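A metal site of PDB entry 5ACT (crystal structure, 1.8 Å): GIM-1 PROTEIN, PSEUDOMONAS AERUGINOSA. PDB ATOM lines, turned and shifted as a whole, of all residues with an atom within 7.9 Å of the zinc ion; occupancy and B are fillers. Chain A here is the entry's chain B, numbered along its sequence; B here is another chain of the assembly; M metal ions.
The backbone NH (N) of His 156 sits at hydrogen-bond distance from the side-chain amide oxygen (OD1) of Asn 160, at 2.8 Å.
ND1 of His 94 lies within hydrogen-bond range of OG1 of Thr 93, at 3.0 Å.
OD2 of Asp 190 is in hydrogen-bond range of NE2 of His 96, at 2.6 Å.
The zinc ion is bound by a ring nitrogen (NE2) of His 156, the side-chain carboxylate of Glu 43 of chain B, a ring nitrogen (ND1) of His 96 and a ring nitrogen (NE2) of His 94.
The zinc ion has four donor atoms within binding distance.
Slightly farther from the zinc ion lies OE1 of Glu 43 of chain B (2.8 Å).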
ATOM      1  N   THR A  93     -19.294   6.015  -3.581  1.00  0.00           N
ATOM      2  CA  THR A  93     -19.121   4.792  -4.309  1.00  0.00           C
ATOM      3  C   THR A  93     -17.870   4.023  -3.875  1.00  0.00           C
ATOM      4  O   THR A  93     -17.774   2.834  -4.122  1.00  0.00           O
ATOM      5  CB  THR A  93     -19.072   5.059  -5.830  1.00  0.00           C
ATOM      6  OG1 THR A  93     -18.005   5.989  -6.126  1.00  0.00           O
ATOM      7  CG2 THR A  93     -20.333   5.626  -6.292  1.00  0.00           C
ATOM      8  N   HIS A  94     -16.933   4.695  -3.202  1.00  0.00           N
ATOM      9  CA  HIS A  94     -15.769   4.028  -2.640  1.00  0.00           C
ATOM     10  C   HIS A  94     -14.983   4.963  -1.714  1.00  0.00           C
ATOM     11  O   HIS A  94     -15.383   6.089  -1.499  1.00  0.00           O
ATOM     12  CB  HIS A  94     -14.840   3.457  -3.729  1.00  0.00           C
ATOM     13  CG  HIS A  94     -14.322   4.464  -4.705  1.00  0.00           C
ATOM     14  ND1 HIS A  94     -15.135   5.326  -5.415  1.00  0.00           N
ATOM     15  CD2 HIS A  94     -13.059   4.700  -5.142  1.00  0.00           C
ATOM     16  CE1 HIS A  94     -14.394   6.051  -6.235  1.00  0.00           C
ATOM     17  NE2 HIS A  94     -13.144   5.694  -6.076  1.00  0.00           N
ATOM     18  N   SER A  95     -13.853   4.465  -1.197  1.00  0.00           N
ATOM     19  CA  SER A  95     -13.179   5.066  -0.048  1.00  0.00           C
ATOM     20  C   SER A  95     -12.079   6.068  -0.405  1.00  0.00           C
ATOM     21  O   SER A  95     -11.553   6.726   0.480  1.00  0.00           O
ATOM     22  CB  SER A  95     -12.570   3.970   0.803  1.00  0.00           C
ATOM     23  OG  SER A  95     -11.496   3.391   0.086  1.00  0.00           O
ATOM     24  N   HIS A  96     -11.728   6.182  -1.678  1.00  0.00           N
ATOM     25  CA  HIS A  96     -10.676   7.104  -2.106  1.00  0.00           C
ATOM     26  C   HIS A  96     -10.791   8.548  -1.560  1.00  0.00           C
ATOM     27  O   HIS A  96     -11.874   8.990  -1.129  1.00  0.00           O
ATOM     28  CB  HIS A  96     -10.643   7.134  -3.647  1.00  0.00           C
ATOM     29  CG  HIS A  96      -9.727   6.096  -4.237  1.00  0.00           C
ATOM     30  ND1 HIS A  96      -9.729   5.780  -5.580  1.00  0.00           N
ATOM     31  CD2 HIS A  96      -8.759   5.330  -3.675  1.00  0.00           C
ATOM     32  CE1 HIS A  96      -8.806   4.863  -5.817  1.00  0.00           C
ATOM     33  NE2 HIS A  96      -8.209   4.567  -4.679  1.00  0.00           N
ATOM     34  N   GLU A  97      -9.645   9.249  -1.596  1.00  0.00           N
ATOM     35  CA  GLU A  97      -9.471  10.559  -0.973  1.00  0.00           C
ATOM     36  C   GLU A  97     -10.585  11.551  -1.301  1.00  0.00           C
ATOM     37  O   GLU A  97     -11.108  12.230  -0.409  1.00  0.00           O
ATOM     38  CB  GLU A  97      -8.122  11.154  -1.398  1.00  0.00           C
ATOM     39  CG  GLU A  97      -7.815  12.553  -0.861  1.00  0.00           C
ATOM     40  CD  GLU A  97      -7.566  12.590   0.636  1.00  0.00           C
ATOM     41  OE1 GLU A  97      -7.005  11.613   1.186  1.00  0.00           O
ATOM     42  OE2 GLU A  97      -7.931  13.606   1.260  1.00  0.00           O
ATOM     43  N   ASP A  98     -10.930  11.637  -2.570  1.00  0.00           N
ATOM     44  CA  ASP A  98     -11.938  12.590  -3.053  1.00  0.00           C
ATOM     45  C   ASP A  98     -13.341  12.309  -2.571  1.00  0.00           C
ATOM     46  O   ASP A  98     -14.215  13.166  -2.718  1.00  0.00           O
ATOM     47  CB  ASP A  98     -11.949  12.612  -4.571  1.00  0.00           C
ATOM     48  CG  ASP A  98     -10.726  13.279  -5.171  1.00  0.00           C
ATOM     49  OD1 ASP A  98      -9.799  13.679  -4.431  1.00  0.00           O
ATOM     50  OD2 ASP A  98     -10.694  13.404  -6.389  1.00  0.00           O
ATOM     51  N   ARG A  99     -13.584  11.119  -2.036  1.00  0.00           N
ATOM     52  CA  ARG A  99     -14.940  10.769  -1.563  1.00  0.00           C
ATOM     53  C   ARG A  99     -15.127  10.995  -0.062  1.00  0.00           C
ATOM     54  O   ARG A  99     -16.148  10.642   0.489  1.00  0.00           O
ATOM     55  CB  ARG A  99     -15.251   9.300  -1.908  1.00  0.00           C
ATOM     56  CG  ARG A  99     -15.177   8.971  -3.418  1.00  0.00           C
ATOM     57  CD  ARG A  99     -15.734  10.151  -4.189  1.00  0.00           C
ATOM     58  NE  ARG A  99     -15.814  10.002  -5.630  1.00  0.00           N
ATOM     59  CZ  ARG A  99     -16.016  11.029  -6.449  1.00  0.00           C
ATOM     60  NH1 ARG A  99     -16.134  12.252  -5.934  1.00  0.00           N
ATOM     61  NH2 ARG A  99     -16.080  10.851  -7.762  1.00  0.00           N
ATOM     62  N   HIS A 156     -11.901  -0.516 -10.441  1.00  0.00           N
ATOM     63  CA  HIS A 156     -11.205   0.742 -10.114  1.00  0.00           C
ATOM     64  C   HIS A 156     -10.581   0.610  -8.724  1.00  0.00           C
ATOM     65  O   HIS A 156      -9.419   0.933  -8.520  1.00  0.00           O
ATOM     66  CB  HIS A 156     -12.200   1.922 -10.204  1.00  0.00           C
ATOM     67  CG  HIS A 156     -11.699   3.211  -9.609  1.00  0.00           C
ATOM     68  ND1 HIS A 156     -10.557   3.862 -10.048  1.00  0.00           N
ATOM     69  CD2 HIS A 156     -12.233   3.996  -8.647  1.00  0.00           C
ATOM     70  CE1 HIS A 156     -10.395   4.964  -9.340  1.00  0.00           C
ATOM     71  NE2 HIS A 156     -11.419   5.086  -8.500  1.00  0.00           N
ATOM     72  N   THR A 157     -11.374   0.104  -7.763  1.00  0.00           N
ATOM     73  CA  THR A 157     -10.901  -0.199  -6.428  1.00  0.00           C
ATOM     74  C   THR A 157     -11.542  -1.511  -5.953  1.00  0.00           C
ATOM     75  O   THR A 157     -12.410  -2.066  -6.640  1.00  0.00           O
ATOM     76  CB  THR A 157     -11.232   0.934  -5.389  1.00  0.00           C
ATOM     77  OG1 THR A 157     -12.646   1.136  -5.332  1.00  0.00           O
ATOM     78  CG2 THR A 157     -10.505   2.241  -5.707  1.00  0.00           C
ATOM     79  N   ASP A 159     -13.542  -2.010  -3.557  1.00  0.00           N
ATOM     80  CA  ASP A 159     -14.834  -1.794  -2.950  1.00  0.00           C
ATOM     81  C   ASP A 159     -15.842  -1.075  -3.829  1.00  0.00           C
ATOM     82  O   ASP A 159     -16.985  -0.871  -3.410  1.00  0.00           O
ATOM     83  CB  ASP A 159     -14.667  -0.985  -1.658  1.00  0.00           C
ATOM     84  CG  ASP A 159     -14.001   0.372  -1.881  1.00  0.00           C
ATOM     85  OD1 ASP A 159     -13.133   0.490  -2.775  1.00  0.00           O
ATOM     86  OD2 ASP A 159     -14.335   1.314  -1.114  1.00  0.00           O
ATOM     87  N   ASN A 160     -15.443  -0.667  -5.030  1.00  0.00           N
ATOM     88  CA  ASN A 160     -16.332   0.203  -5.819  1.00  0.00           C
ATOM     89  C   ASN A 160     -17.738  -0.361  -6.053  1.00  0.00           C
ATOM     90  O   ASN A 160     -17.907  -1.520  -6.468  1.00  0.00           O
ATOM     91  CB  ASN A 160     -15.711   0.567  -7.174  1.00  0.00           C
ATOM     92  CG  ASN A 160     -15.105  -0.621  -7.943  1.00  0.00           C
ATOM     93  OD1 ASN A 160     -14.099  -0.450  -8.659  1.00  0.00           O
ATOM     94  ND2 ASN A 160     -15.709  -1.815  -7.815  1.00  0.00           N
ATOM     95  N   GLY A 174     -19.529   5.685 -11.749  1.00  0.00           N
ATOM     96  CA  GLY A 174     -18.392   6.271 -11.070  1.00  0.00           C
ATOM     97  C   GLY A 174     -17.116   5.880 -11.821  1.00  0.00           C
ATOM     98  O   GLY A 174     -17.144   5.715 -13.025  1.00  0.00           O
ATOM     99  N   OCS A 175     -16.032   5.681 -11.099  1.00  0.00           N
ATOM    100  CA  OCS A 175     -14.737   5.413 -11.777  1.00  0.00           C
ATOM    101  CB  OCS A 175     -13.550   5.936 -10.956  1.00  0.00           C
ATOM    102  SG  OCS A 175     -13.131   7.620 -11.465  1.00  0.00           S
ATOM    103  C   OCS A 175     -14.540   3.975 -12.205  1.00  0.00           C
ATOM    104  O   OCS A 175     -13.514   3.629 -12.827  1.00  0.00           O
ATOM    105  OD1 OCS A 175     -12.910   7.624 -12.879  1.00  0.00           O
ATOM    106  OD2 OCS A 175     -12.007   8.058 -10.742  1.00  0.00           O
ATOM    107  OD3 OCS A 175     -14.243   8.466 -11.138  1.00  0.00           O
ATOM    108  N   LEU A 176     -15.514   3.130 -11.883  1.00  0.00           N
ATOM    109  CA  LEU A 176     -15.547   1.753 -12.341  1.00  0.00           C
ATOM    110  C   LEU A 176     -15.815   1.706 -13.838  1.00  0.00           C
ATOM    111  O   LEU A 176     -15.472   0.722 -14.516  1.00  0.00           O
ATOM    112  CB  LEU A 176     -16.599   0.951 -11.592  1.00  0.00           C
ATOM    113  CG  LEU A 176     -16.769  -0.525 -11.956  1.00  0.00           C
ATOM    114  CD1 LEU A 176     -15.459  -1.326 -11.911  1.00  0.00           C
ATOM    115  CD2 LEU A 176     -17.820  -1.093 -10.989  1.00  0.00           C
ATOM    116  N   TYR A 187      -6.921   6.427 -12.825  1.00  0.00           N
ATOM    117  CA  TYR A 187      -5.992   6.144 -11.724  1.00  0.00           C
ATOM    118  C   TYR A 187      -6.115   4.697 -11.265  1.00  0.00           C
ATOM    119  O   TYR A 187      -7.127   4.317 -10.658  1.00  0.00           O
ATOM    120  CB  TYR A 187      -6.216   7.102 -10.547  1.00  0.00           C
ATOM    121  CG  TYR A 187      -5.425   6.675  -9.341  1.00  0.00           C
ATOM    122  CD1 TYR A 187      -4.034   6.602  -9.393  1.00  0.00           C
ATOM    123  CD2 TYR A 187      -6.061   6.305  -8.157  1.00  0.00           C
ATOM    124  CE1 TYR A 187      -3.302   6.190  -8.313  1.00  0.00           C
ATOM    125  CE2 TYR A 187      -5.333   5.895  -7.064  1.00  0.00           C
ATOM    126  CZ  TYR A 187      -3.943   5.836  -7.146  1.00  0.00           C
ATOM    127  OH  TYR A 187      -3.203   5.421  -6.056  1.00  0.00           O
ATOM    128  N   ASP A 190      -5.016   1.590  -6.990  1.00  0.00           N
ATOM    129  CA  ASP A 190      -5.694   0.651  -6.089  1.00  0.00           C
ATOM    130  C   ASP A 190      -6.597  -0.317  -6.842  1.00  0.00           C
ATOM    131  O   ASP A 190      -7.372  -1.056  -6.227  1.00  0.00           O
ATOM    132  CB  ASP A 190      -6.504   1.420  -5.039  1.00  0.00           C
ATOM    133  CG  ASP A 190      -5.623   2.320  -4.184  1.00  0.00           C
ATOM    134  OD1 ASP A 190      -4.714   1.772  -3.515  1.00  0.00           O
ATOM    135  OD2 ASP A 190      -5.826   3.564  -4.216  1.00  0.00           O
ATOM    136  N   GLU B  43      -7.084  11.260  -9.713  1.00  0.00           N
ATOM    137  CA  GLU B  43      -8.323  10.518  -9.773  1.00  0.00           C
ATOM    138  C   GLU B  43      -9.034  10.862 -11.065  1.00  0.00           C
ATOM    139  O   GLU B  43      -9.147  12.032 -11.444  1.00  0.00           O
ATOM    140  CB  GLU B  43      -9.201  10.820  -8.559  1.00  0.00           C
ATOM    141  CG  GLU B  43     -10.554  10.105  -8.585  1.00  0.00           C
ATOM    142  CD  GLU B  43     -10.487   8.666  -8.054  1.00  0.00           C
ATOM    143  OE1 GLU B  43      -9.477   7.963  -8.290  1.00  0.00           O
ATOM    144  OE2 GLU B  43     -11.483   8.232  -7.415  1.00  0.00           O
ATOM    145  N   GLY B  44      -9.511   9.835 -11.752  1.00  0.00           N
ATOM    146  CA  GLY B  44     -10.203  10.035 -13.005  1.00  0.00           C
ATOM    147  C   GLY B  44      -9.289   9.977 -14.224  1.00  0.00           C
ATOM    148  O   GLY B  44      -9.751   9.641 -15.318  1.00  0.00           O
HETATM  149 ZN    ZN M   1     -11.245   6.286  -6.941  1.00  0.00          ZN
